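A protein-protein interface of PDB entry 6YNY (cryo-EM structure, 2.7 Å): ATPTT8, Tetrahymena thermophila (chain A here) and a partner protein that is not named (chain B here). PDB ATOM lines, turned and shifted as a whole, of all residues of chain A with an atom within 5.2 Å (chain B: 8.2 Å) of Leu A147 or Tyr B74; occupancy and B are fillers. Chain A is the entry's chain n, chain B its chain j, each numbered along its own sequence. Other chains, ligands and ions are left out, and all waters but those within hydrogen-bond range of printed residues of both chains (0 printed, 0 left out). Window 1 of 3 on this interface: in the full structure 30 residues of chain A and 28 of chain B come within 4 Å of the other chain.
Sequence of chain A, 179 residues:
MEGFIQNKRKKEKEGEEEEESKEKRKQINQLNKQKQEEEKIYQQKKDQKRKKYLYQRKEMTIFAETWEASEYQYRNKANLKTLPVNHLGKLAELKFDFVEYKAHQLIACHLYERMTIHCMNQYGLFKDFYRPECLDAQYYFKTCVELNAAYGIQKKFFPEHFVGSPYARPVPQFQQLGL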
ATOM      1  N   LYS A  81      20.576  35.547 -33.275  1.00  0.00           N
ATOM      2  CA  LYS A  81      20.695  34.903 -31.979  1.00  0.00           C
ATOM      3  C   LYS A  81      21.214  35.900 -30.959  1.00  0.00           C
ATOM      4  O   LYS A  81      21.925  36.848 -31.298  1.00  0.00           O
ATOM      5  CB  LYS A  81      21.635  33.698 -32.015  1.00  0.00           C
ATOM      6  CG  LYS A  81      21.040  32.451 -32.595  1.00  0.00           C
ATOM      7  CD  LYS A  81      21.883  31.253 -32.236  1.00  0.00           C
ATOM      8  CE  LYS A  81      21.392  29.994 -32.911  1.00  0.00           C
ATOM      9  NZ  LYS A  81      19.972  29.717 -32.613  1.00  0.00           N
ATOM     10  N   THR A  82      20.843  35.673 -29.708  1.00  0.00           N
ATOM     11  CA  THR A  82      21.402  36.378 -28.572  1.00  0.00           C
ATOM     12  C   THR A  82      22.129  35.381 -27.680  1.00  0.00           C
ATOM     13  O   THR A  82      22.021  34.164 -27.848  1.00  0.00           O
ATOM     14  CB  THR A  82      20.321  37.105 -27.768  1.00  0.00           C
ATOM     15  OG1 THR A  82      19.295  36.180 -27.392  1.00  0.00           O
ATOM     16  CG2 THR A  82      19.722  38.224 -28.572  1.00  0.00           C
ATOM     17  N   LEU A  83      22.878  35.916 -26.733  1.00  0.00           N
ATOM     18  CA  LEU A  83      23.540  35.107 -25.724  1.00  0.00           C
ATOM     19  C   LEU A  83      22.902  35.430 -24.380  1.00  0.00           C
ATOM     20  O   LEU A  83      23.465  36.199 -23.591  1.00  0.00           O
ATOM     21  CB  LEU A  83      25.041  35.378 -25.712  1.00  0.00           C
ATOM     22  CG  LEU A  83      25.916  34.347 -25.010  1.00  0.00           C
ATOM     23  CD1 LEU A  83      25.936  33.040 -25.779  1.00  0.00           C
ATOM     24  CD2 LEU A  83      27.306  34.895 -24.864  1.00  0.00           C
ATOM     25  N   PRO A  84      21.731  34.876 -24.089  1.00  0.00           N
ATOM     26  CA  PRO A  84      20.983  35.306 -22.906  1.00  0.00           C
ATOM     27  C   PRO A  84      21.592  34.778 -21.620  1.00  0.00           C
ATOM     28  O   PRO A  84      22.425  33.871 -21.602  1.00  0.00           O
ATOM     29  CB  PRO A  84      19.595  34.714 -23.140  1.00  0.00           C
ATOM     30  CG  PRO A  84      19.853  33.505 -23.935  1.00  0.00           C
ATOM     31  CD  PRO A  84      21.030  33.806 -24.814  1.00  0.00           C
ATOM     32  N   TYR A 112      22.334  25.333 -15.544  1.00  0.00           N
ATOM     33  CA  TYR A 112      21.781  24.197 -16.270  1.00  0.00           C
ATOM     34  C   TYR A 112      22.545  22.921 -15.961  1.00  0.00           C
ATOM     35  O   TYR A 112      21.969  21.829 -15.986  1.00  0.00           O
ATOM     36  CB  TYR A 112      21.804  24.470 -17.770  1.00  0.00           C
ATOM     37  CG  TYR A 112      21.123  25.749 -18.177  1.00  0.00           C
ATOM     38  CD1 TYR A 112      19.958  26.159 -17.561  1.00  0.00           C
ATOM     39  CD2 TYR A 112      21.648  26.546 -19.176  1.00  0.00           C
ATOM     40  CE1 TYR A 112      19.334  27.323 -17.928  1.00  0.00           C
ATOM     41  CE2 TYR A 112      21.032  27.709 -19.550  1.00  0.00           C
ATOM     42  CZ  TYR A 112      19.874  28.096 -18.926  1.00  0.00           C
ATOM     43  OH  TYR A 112      19.258  29.262 -19.302  1.00  0.00           O
ATOM     44  N   TYR A 139      19.413  19.662 -22.238  1.00  0.00           N
ATOM     45  CA  TYR A 139      19.549  20.251 -23.564  1.00  0.00           C
ATOM     46  C   TYR A 139      20.083  21.674 -23.484  1.00  0.00           C
ATOM     47  O   TYR A 139      20.927  22.071 -24.293  1.00  0.00           O
ATOM     48  CB  TYR A 139      18.204  20.220 -24.286  1.00  0.00           C
ATOM     49  CG  TYR A 139      18.204  20.938 -25.610  1.00  0.00           C
ATOM     50  CD1 TYR A 139      18.818  20.387 -26.719  1.00  0.00           C
ATOM     51  CD2 TYR A 139      17.587  22.167 -25.751  1.00  0.00           C
ATOM     52  CE1 TYR A 139      18.823  21.039 -27.924  1.00  0.00           C
ATOM     53  CE2 TYR A 139      17.587  22.827 -26.954  1.00  0.00           C
ATOM     54  CZ  TYR A 139      18.207  22.258 -28.038  1.00  0.00           C
ATOM     55  OH  TYR A 139      18.208  22.914 -29.242  1.00  0.00           O
ATOM     56  N   TYR A 140      19.600  22.456 -22.518  1.00  0.00           N
ATOM     57  CA  TYR A 140      20.108  23.809 -22.344  1.00  0.00           C
ATOM     58  C   TYR A 140      21.589  23.801 -21.996  1.00  0.00           C
ATOM     59  O   TYR A 140      22.357  24.634 -22.488  1.00  0.00           O
ATOM     60  CB  TYR A 140      19.315  24.533 -21.261  1.00  0.00           C
ATOM     61  CG  TYR A 140      18.004  25.125 -21.714  1.00  0.00           C
ATOM     62  CD1 TYR A 140      17.367  24.682 -22.861  1.00  0.00           C
ATOM     63  CD2 TYR A 140      17.411  26.147 -20.996  1.00  0.00           C
ATOM     64  CE1 TYR A 140      16.177  25.234 -23.266  1.00  0.00           C
ATOM     65  CE2 TYR A 140      16.229  26.700 -21.393  1.00  0.00           C
ATOM     66  CZ  TYR A 140      15.611  26.243 -22.528  1.00  0.00           C
ATOM     67  OH  TYR A 140      14.424  26.805 -22.924  1.00  0.00           O
ATOM     68  N   THR A 143      23.604  22.845 -24.981  1.00  0.00           N
ATOM     69  CA  THR A 143      23.531  23.889 -25.991  1.00  0.00           C
ATOM     70  C   THR A 143      24.232  25.163 -25.546  1.00  0.00           C
ATOM     71  O   THR A 143      24.801  25.874 -26.380  1.00  0.00           O
ATOM     72  CB  THR A 143      22.069  24.200 -26.320  1.00  0.00           C
ATOM     73  OG1 THR A 143      21.403  23.005 -26.742  1.00  0.00           O
ATOM     74  CG2 THR A 143      21.971  25.227 -27.412  1.00  0.00           C
ATOM     75  N   CYS A 144      24.199  25.463 -24.250  1.00  0.00           N
ATOM     76  CA  CYS A 144      24.827  26.678 -23.748  1.00  0.00           C
ATOM     77  C   CYS A 144      26.339  26.624 -23.908  1.00  0.00           C
ATOM     78  O   CYS A 144      26.962  27.610 -24.316  1.00  0.00           O
ATOM     79  CB  CYS A 144      24.440  26.888 -22.285  1.00  0.00           C
ATOM     80  SG  CYS A 144      24.940  28.447 -21.552  1.00  0.00           S
ATOM     81  N   VAL A 145      26.949  25.478 -23.599  1.00  0.00           N
ATOM     82  CA  VAL A 145      28.396  25.357 -23.692  1.00  0.00           C
ATOM     83  C   VAL A 145      28.859  25.255 -25.135  1.00  0.00           C
ATOM     84  O   VAL A 145      30.023  25.544 -25.429  1.00  0.00           O
ATOM     85  CB  VAL A 145      28.894  24.149 -22.875  1.00  0.00           C
ATOM     86  CG1 VAL A 145      28.477  24.285 -21.442  1.00  0.00           C
ATOM     87  CG2 VAL A 145      28.370  22.857 -23.441  1.00  0.00           C
ATOM     88  N   GLU A 146      27.978  24.851 -26.047  1.00  0.00           N
ATOM     89  CA  GLU A 146      28.334  24.810 -27.458  1.00  0.00           C
ATOM     90  C   GLU A 146      28.325  26.202 -28.072  1.00  0.00           C
ATOM     91  O   GLU A 146      29.246  26.564 -28.810  1.00  0.00           O
ATOM     92  CB  GLU A 146      27.375  23.891 -28.208  1.00  0.00           C
ATOM     93  CG  GLU A 146      27.603  22.427 -27.934  1.00  0.00           C
ATOM     94  CD  GLU A 146      26.570  21.541 -28.600  1.00  0.00           C
ATOM     95  OE1 GLU A 146      25.502  22.059 -28.985  1.00  0.00           O
ATOM     96  OE2 GLU A 146      26.824  20.328 -28.737  1.00  0.00           O
ATOM     97  N   LEU A 147      27.292  26.992 -27.780  1.00  0.00           N
ATOM     98  CA  LEU A 147      27.242  28.361 -28.275  1.00  0.00           C
ATOM     99  C   LEU A 147      28.336  29.210 -27.650  1.00  0.00           C
ATOM    100  O   LEU A 147      29.021  29.971 -28.343  1.00  0.00           O
ATOM    101  CB  LEU A 147      25.872  28.967 -27.987  1.00  0.00           C
ATOM    102  CG  LEU A 147      24.685  28.397 -28.752  1.00  0.00           C
ATOM    103  CD1 LEU A 147      23.407  28.905 -28.145  1.00  0.00           C
ATOM    104  CD2 LEU A 147      24.767  28.778 -30.212  1.00  0.00           C
ATOM    105  N   ASN A 148      28.514  29.097 -26.335  1.00  0.00           N
ATOM    106  CA  ASN A 148      29.521  29.904 -25.658  1.00  0.00           C
ATOM    107  C   ASN A 148      30.926  29.565 -26.132  1.00  0.00           C
ATOM    108  O   ASN A 148      31.789  30.445 -26.189  1.00  0.00           O
ATOM    109  CB  ASN A 148      29.398  29.725 -24.149  1.00  0.00           C
ATOM    110  CG  ASN A 148      28.391  30.669 -23.536  1.00  0.00           C
ATOM    111  OD1 ASN A 148      28.722  31.793 -23.165  1.00  0.00           O
ATOM    112  ND2 ASN A 148      27.152  30.222 -23.435  1.00  0.00           N
ATOM    113  N   ALA A 149      31.174  28.302 -26.474  1.00  0.00           N
ATOM    114  CA  ALA A 149      32.463  27.944 -27.053  1.00  0.00           C
ATOM    115  C   ALA A 149      32.640  28.572 -28.427  1.00  0.00           C
ATOM    116  O   ALA A 149      33.746  28.984 -28.792  1.00  0.00           O
ATOM    117  CB  ALA A 149      32.596  26.428 -27.144  1.00  0.00           C
ATOM    118  N   ALA A 150      31.560  28.659 -29.202  1.00  0.00           N
ATOM    119  CA  ALA A 150      31.646  29.265 -30.524  1.00  0.00           C
ATOM    120  C   ALA A 150      31.751  30.780 -30.435  1.00  0.00           C
ATOM    121  O   ALA A 150      32.552  31.394 -31.147  1.00  0.00           O
ATOM    122  CB  ALA A 150      30.439  28.857 -31.360  1.00  0.00           C
ATOM    123  N   TYR A 151      30.947  31.403 -29.575  1.00  0.00           N
ATOM    124  CA  TYR A 151      31.061  32.843 -29.385  1.00  0.00           C
ATOM    125  C   TYR A 151      32.401  33.220 -28.772  1.00  0.00           C
ATOM    126  O   TYR A 151      32.953  34.276 -29.096  1.00  0.00           O
ATOM    127  CB  TYR A 151      29.921  33.350 -28.507  1.00  0.00           C
ATOM    128  CG  TYR A 151      28.646  33.642 -29.255  1.00  0.00           C
ATOM    129  CD1 TYR A 151      28.520  34.788 -30.019  1.00  0.00           C
ATOM    130  CD2 TYR A 151      27.563  32.784 -29.183  1.00  0.00           C
ATOM    131  CE1 TYR A 151      27.363  35.066 -30.697  1.00  0.00           C
ATOM    132  CE2 TYR A 151      26.396  33.055 -29.859  1.00  0.00           C
ATOM    133  CZ  TYR A 151      26.302  34.199 -30.614  1.00  0.00           C
ATOM    134  OH  TYR A 151      25.141  34.475 -31.291  1.00  0.00           O
ATOM    135  N   GLY A 152      32.934  32.380 -27.887  1.00  0.00           N
ATOM    136  CA  GLY A 152      34.226  32.669 -27.294  1.00  0.00           C
ATOM    137  C   GLY A 152      35.351  32.626 -28.308  1.00  0.00           C
ATOM    138  O   GLY A 152      36.249  33.470 -28.289  1.00  0.00           O
ATOM    139  N   PRO B  71      12.556  19.319 -27.239  1.00  0.00           N
ATOM    140  CA  PRO B  71      12.801  20.261 -26.147  1.00  0.00           C
ATOM    141  C   PRO B  71      12.428  21.681 -26.537  1.00  0.00           C
ATOM    142  O   PRO B  71      12.335  22.028 -27.716  1.00  0.00           O
ATOM    143  CB  PRO B  71      14.308  20.134 -25.901  1.00  0.00           C
ATOM    144  CG  PRO B  71      14.692  18.847 -26.483  1.00  0.00           C
ATOM    145  CD  PRO B  71      13.783  18.612 -27.633  1.00  0.00           C
ATOM    146  N   ASN B  72      12.205  22.505 -25.526  1.00  0.00           N
ATOM    147  CA  ASN B  72      12.010  23.921 -25.775  1.00  0.00           C
ATOM    148  C   ASN B  72      13.282  24.496 -26.388  1.00  0.00           C
ATOM    149  O   ASN B  72      14.378  24.240 -25.874  1.00  0.00           O
ATOM    150  CB  ASN B  72      11.669  24.675 -24.493  1.00  0.00           C
ATOM    151  CG  ASN B  72      10.204  24.613 -24.152  1.00  0.00           C
ATOM    152  OD1 ASN B  72       9.368  25.174 -24.857  1.00  0.00           O
ATOM    153  ND2 ASN B  72       9.883  23.949 -23.051  1.00  0.00           N
ATOM    154  N   PRO B  73      13.190  25.256 -27.474  1.00  0.00           N
ATOM    155  CA  PRO B  73      14.400  25.833 -28.056  1.00  0.00           C
ATOM    156  C   PRO B  73      15.126  26.712 -27.053  1.00  0.00           C
ATOM    157  O   PRO B  73      14.513  27.373 -26.212  1.00  0.00           O
ATOM    158  CB  PRO B  73      13.873  26.640 -29.246  1.00  0.00           C
ATOM    159  CG  PRO B  73      12.447  26.840 -28.982  1.00  0.00           C
ATOM    160  CD  PRO B  73      11.989  25.653 -28.223  1.00  0.00           C
ATOM    161  N   TYR B  74      16.447  26.695 -27.138  1.00  0.00           N
ATOM    162  CA  TYR B  74      17.258  27.519 -26.260  1.00  0.00           C
ATOM    163  C   TYR B  74      16.792  28.972 -26.343  1.00  0.00           C
ATOM    164  O   TYR B  74      16.519  29.470 -27.443  1.00  0.00           O
ATOM    165  CB  TYR B  74      18.733  27.401 -26.644  1.00  0.00           C
ATOM    166  CG  TYR B  74      19.680  28.086 -25.696  1.00  0.00           C
ATOM    167  CD1 TYR B  74      20.082  27.472 -24.525  1.00  0.00           C
ATOM    168  CD2 TYR B  74      20.183  29.340 -25.979  1.00  0.00           C
ATOM    169  CE1 TYR B  74      20.943  28.093 -23.660  1.00  0.00           C
ATOM    170  CE2 TYR B  74      21.048  29.968 -25.121  1.00  0.00           C
ATOM    171  CZ  TYR B  74      21.428  29.340 -23.964  1.00  0.00           C
ATOM    172  OH  TYR B  74      22.291  29.972 -23.107  1.00  0.00           O
ATOM    173  N   PRO B  75      16.671  29.671 -25.218  1.00  0.00           N
ATOM    174  CA  PRO B  75      16.101  31.022 -25.251  1.00  0.00           C
ATOM    175  C   PRO B  75      16.835  31.933 -26.222  1.00  0.00           C
ATOM    176  O   PRO B  75      18.065  31.994 -26.243  1.00  0.00           O
ATOM    177  CB  PRO B  75      16.242  31.501 -23.801  1.00  0.00           C
ATOM    178  CG  PRO B  75      17.181  30.563 -23.160  1.00  0.00           C
ATOM    179  CD  PRO B  75      17.011  29.271 -23.846  1.00  0.00           C
ATOM    180  N   ASN B  76      16.056  32.640 -27.035  1.00  0.00           N
ATOM    181  CA  ASN B  76      16.579  33.567 -28.028  1.00  0.00           C
ATOM    182  C   ASN B  76      15.697  34.803 -28.034  1.00  0.00           C
ATOM    183  O   ASN B  76      14.489  34.704 -28.267  1.00  0.00           O
ATOM    184  CB  ASN B  76      16.615  32.920 -29.411  1.00  0.00           C
ATOM    185  CG  ASN B  76      17.284  33.785 -30.445  1.00  0.00           C
ATOM    186  OD1 ASN B  76      17.457  34.987 -30.255  1.00  0.00           O
ATOM    187  ND2 ASN B  76      17.657  33.179 -31.556  1.00  0.00           N
ATOM    188  N   GLY B  77      16.295  35.960 -27.772  1.00  0.00           N
ATOM    189  CA  GLY B  77      15.545  37.196 -27.726  1.00  0.00           C
ATOM    190  C   GLY B  77      15.227  37.802 -29.070  1.00  0.00           C
ATOM    191  O   GLY B  77      14.415  38.729 -29.139  1.00  0.00           O
ATOM    192  N   TYR B  88       9.232  40.709 -26.429  1.00  0.00           N
ATOM    193  CA  TYR B  88       9.392  39.299 -26.113  1.00  0.00           C
ATOM    194  C   TYR B  88      10.598  39.083 -25.214  1.00  0.00           C
ATOM    195  O   TYR B  88      11.700  39.555 -25.505  1.00  0.00           O
ATOM    196  CB  TYR B  88       9.538  38.488 -27.397  1.00  0.00           C
ATOM    197  CG  TYR B  88       9.884  37.039 -27.170  1.00  0.00           C
ATOM    198  CD1 TYR B  88       8.982  36.176 -26.578  1.00  0.00           C
ATOM    199  CD2 TYR B  88      11.112  36.532 -27.557  1.00  0.00           C
ATOM    200  CE1 TYR B  88       9.292  34.857 -26.371  1.00  0.00           C
ATOM    201  CE2 TYR B  88      11.429  35.213 -27.353  1.00  0.00           C
ATOM    202  CZ  TYR B  88      10.516  34.379 -26.762  1.00  0.00           C
ATOM    203  OH  TYR B  88      10.829  33.059 -26.557  1.00  0.00           O
ATOM    204  N   PRO B  90      12.456  35.774 -23.684  1.00  0.00           N
ATOM    205  CA  PRO B  90      12.455  34.306 -23.631  1.00  0.00           C
ATOM    206  C   PRO B  90      12.652  33.744 -22.237  1.00  0.00           C
ATOM    207  O   PRO B  90      12.475  32.535 -22.049  1.00  0.00           O
ATOM    208  CB  PRO B  90      13.618  33.926 -24.550  1.00  0.00           C
ATOM    209  CG  PRO B  90      14.516  35.088 -24.516  1.00  0.00           C
ATOM    210  CD  PRO B  90      13.648  36.293 -24.371  1.00  0.00           C
ATOM    211  N   LEU B  91      13.011  34.573 -21.264  1.00  0.00           N
ATOM    212  CA  LEU B  91      13.231  34.137 -19.896  1.00  0.00           C
ATOM    213  C   LEU B  91      12.019  34.351 -19.006  1.00  0.00           C
ATOM    214  O   LEU B  91      12.067  34.004 -17.823  1.00  0.00           O
ATOM    215  CB  LEU B  91      14.433  34.871 -19.308  1.00  0.00           C
ATOM    216  CG  LEU B  91      15.705  34.836 -20.150  1.00  0.00           C
ATOM    217  CD1 LEU B  91      16.763  35.701 -19.525  1.00  0.00           C
ATOM    218  CD2 LEU B  91      16.214  33.423 -20.311  1.00  0.00           C
ATOM    219  N   ARG B  96       7.924  28.119 -24.720  1.00  0.00           N
ATOM    220  CA  ARG B  96       7.719  29.169 -25.707  1.00  0.00           C
ATOM    221  C   ARG B  96       6.354  29.001 -26.357  1.00  0.00           C
ATOM    222  O   ARG B  96       6.051  27.942 -26.915  1.00  0.00           O
ATOM    223  CB  ARG B  96       8.824  29.129 -26.756  1.00  0.00           C
ATOM    224  CG  ARG B  96       8.923  30.392 -27.579  1.00  0.00           C
ATOM    225  CD  ARG B  96      10.086  30.350 -28.538  1.00  0.00           C
ATOM    226  NE  ARG B  96       9.801  29.558 -29.723  1.00  0.00           N
ATOM    227  CZ  ARG B  96      10.615  29.466 -30.764  1.00  0.00           C
ATOM    228  NH1 ARG B  96      11.768  30.117 -30.768  1.00  0.00           N
ATOM    229  NH2 ARG B  96      10.278  28.724 -31.804  1.00  0.00           N
ATOM    230  N   GLY B 109      16.023  28.848 -36.829  1.00  0.00           N
ATOM    231  CA  GLY B 109      16.809  27.846 -36.143  1.00  0.00           C
ATOM    232  C   GLY B 109      16.354  27.590 -34.724  1.00  0.00           C
ATOM    233  O   GLY B 109      17.087  27.868 -33.770  1.00  0.00           O
ATOM    234  N   ASN B 110      15.135  27.068 -34.570  1.00  0.00           N
ATOM    235  CA  ASN B 110      14.668  26.665 -33.249  1.00  0.00           C
ATOM    236  C   ASN B 110      15.679  25.758 -32.569  1.00  0.00           C
ATOM    237  O   ASN B 110      15.954  25.903 -31.373  1.00  0.00           O
ATOM    238  CB  ASN B 110      13.320  25.957 -33.359  1.00  0.00           C
ATOM    239  CG  ASN B 110      12.211  26.882 -33.774  1.00  0.00           C
ATOM    240  OD1 ASN B 110      12.295  28.094 -33.587  1.00  0.00           O
ATOM    241  ND2 ASN B 110      11.155  26.316 -34.333  1.00  0.00           N
ATOM    242  N   TYR B 111      16.247  24.821 -33.319  1.00  0.00           N
ATOM    243  CA  TYR B 111      17.262  23.902 -32.822  1.00  0.00           C
ATOM    244  C   TYR B 111      18.481  24.060 -33.718  1.00  0.00           C
ATOM    245  O   TYR B 111      18.655  23.323 -34.690  1.00  0.00           O
ATOM    246  CB  TYR B 111      16.740  22.476 -32.809  1.00  0.00           C
ATOM    247  CG  TYR B 111      15.370  22.361 -32.195  1.00  0.00           C
ATOM    248  CD1 TYR B 111      15.205  22.310 -30.822  1.00  0.00           C
ATOM    249  CD2 TYR B 111      14.239  22.314 -32.989  1.00  0.00           C
ATOM    250  CE1 TYR B 111      13.959  22.212 -30.262  1.00  0.00           C
ATOM    251  CE2 TYR B 111      12.990  22.215 -32.436  1.00  0.00           C
ATOM    252  CZ  TYR B 111      12.853  22.165 -31.072  1.00  0.00           C
ATOM    253  OH  TYR B 111      11.608  22.067 -30.512  1.00  0.00           O
ATOM    254  N   SER B 112      19.327  25.029 -33.383  1.00  0.00           N
ATOM    255  CA  SER B 112      20.494  25.330 -34.189  1.00  0.00           C
ATOM    256  C   SER B 112      21.619  25.794 -33.284  1.00  0.00           C
ATOM    257  O   SER B 112      21.386  26.307 -32.187  1.00  0.00           O
ATOM    258  CB  SER B 112      20.193  26.400 -35.244  1.00  0.00           C
ATOM    259  OG  SER B 112      19.802  27.617 -34.645  1.00  0.00           O
ATOM    260  N   THR B 113      22.842  25.599 -33.756  1.00  0.00           N
ATOM    261  CA  THR B 113      24.040  26.029 -33.059  1.00  0.00           C
ATOM    262  C   THR B 113      24.925  26.811 -34.016  1.00  0.00           C
ATOM    263  O   THR B 113      24.734  26.799 -35.233  1.00  0.00           O
ATOM    264  CB  THR B 113      24.816  24.839 -32.483  1.00  0.00           C
ATOM    265  OG1 THR B 113      25.257  23.989 -33.546  1.00  0.00           O
ATOM    266  CG2 THR B 113      23.947  24.047 -31.536  1.00  0.00           C
ATOM    267  N   LEU B 114      25.906  27.495 -33.441  1.00  0.00           N
ATOM    268  CA  LEU B 114      26.839  28.317 -34.198  1.00  0.00           C
ATOM    269  C   LEU B 114      28.089  27.503 -34.504  1.00  0.00           C
ATOM    270  O   LEU B 114      28.761  27.019 -33.587  1.00  0.00           O
ATOM    271  CB  LEU B 114      27.185  29.579 -33.417  1.00  0.00           C
ATOM    272  CG  LEU B 114      28.190  30.536 -34.049  1.00  0.00           C
ATOM    273  CD1 LEU B 114      27.696  31.022 -35.385  1.00  0.00           C
ATOM    274  CD2 LEU B 114      28.429  31.693 -33.119  1.00  0.00           C
ATOM    275  N   VAL B 115      28.393  27.348 -35.789  1.00  0.00           N
ATOM    276  CA  VAL B 115      29.568  26.632 -36.247  1.00  0.00           C
ATOM    277  C   VAL B 115      30.299  27.492 -37.270  1.00  0.00           C
ATOM    278  O   VAL B 115      29.846  28.570 -37.650  1.00  0.00           O
ATOM    279  CB  VAL B 115      29.227  25.257 -36.855  1.00  0.00           C
ATOM    280  CG1 VAL B 115      28.487  24.398 -35.865  1.00  0.00           C
ATOM    281  CG2 VAL B 115      28.443  25.426 -38.137  1.00  0.00           C
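O of Pro B73 sits at hydrogen-bond distance from OH of Tyr A140 (3.3 Å). OH of Tyr B74 is in hydrogen-bond range of SG of Cys A144 (3.4 Å). OD1 of Asn B76 sits at hydrogen-bond distance from N of Thr A82, at 3.5 Å. The side-chain hydroxyl (OG1) of Thr A82 lies within hydrogen-bond range of the backbone NH (N) of Gly B77 (3.0 Å). The side-chain hydroxyl (OG) of Ser B112 is in hydrogen-bond range of the side-chain amino group (NZ) of Lys A81 (2.9 Å).
Leu A147 touches just these residues of chain B: Tyr B74 and Leu B114. Tyr B74 touches just these residues of chain A: Pro A84 (3.9 Å), Tyr A140 (3.9 Å), Thr A143 (3.98 Å), Cys A144 (3.4 Å) and Leu A147 (3.9 Å). Printed residues of chain B within 4 Å of Ala A150: Leu B114 (3.3 Å). Of the printed residues of chain B, Cys A144 touches Tyr B74. Printed residues of chain A within 4 Å of Gly B77: Thr A82 (3.0 Å). Printed residues of chain B within 4 Å of Thr A82: Asn B76 and Gly B77. Of the printed residues of chain A, Thr B113 touches Glu A146 (3.6 Å). The nearest residue of chain B that does not touch Leu A147 is Thr B113 (4.02 Å). The nearest printed residue of chain B that does not touch Tyr A139 is Tyr B74 (4.04 Å).
Among the printed residues, merely in contact across the chains: Lys A81 with Asn B76, Lys A81 with Gly B109, Pro A84 with Tyr B74, Pro A84 with Pro B75, Tyr A139 with Pro B71, Tyr A139 with Asn B72, Tyr A139 with Tyr B111, Tyr A140 with Asn B72, Tyr A140 with Tyr B74, Tyr A140 with Pro B75, Thr A143 with Tyr B74, Glu A146 with Thr B113, Leu A147 with Tyr B74, Leu A147 with Leu B114 and Ala A150 with Leu B114.
Of the 18 printed residues of chain B, 12 touch a printed residue of chain A. Printed residues of chain B that touch a printed residue of chain A: Pro B71, Asn B72, Pro B73, Tyr B74, Pro B75, Asn B76, Gly B77, Gly B109, Tyr B111, Ser B112, Thr B113 and Leu B114. Hydrophobic or aromatic side chains of chain B within 4 Å of the printed part of chain A: Pro B71, Tyr B74, Pro B75, Tyr B111 and Leu B114. Among the printed residues, 20 pairs touch across the chains. Among the printed residues, no Asp or Glu carboxylate lies within 4 Å of a Lys or Arg side-chain nitrogen of the other chain.
O of Pro B71 is in hydrogen-bond range of OH of Tyr B111, at 2.9 Å. The side-chain amide oxygen of Asn B72 lies within hydrogen-bond range of the backbone NH of Arg B96 (3.3 Å). O of Gly B109 sits at hydrogen-bond distance from OG of Ser B112 (2.9 Å). O of Tyr A139 is in hydrogen-bond range of OG1 of Thr A143, at 2.7 Å. ND2 of Asn A148 lies within hydrogen-bond range of O of Cys A144 (2.8 Å).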
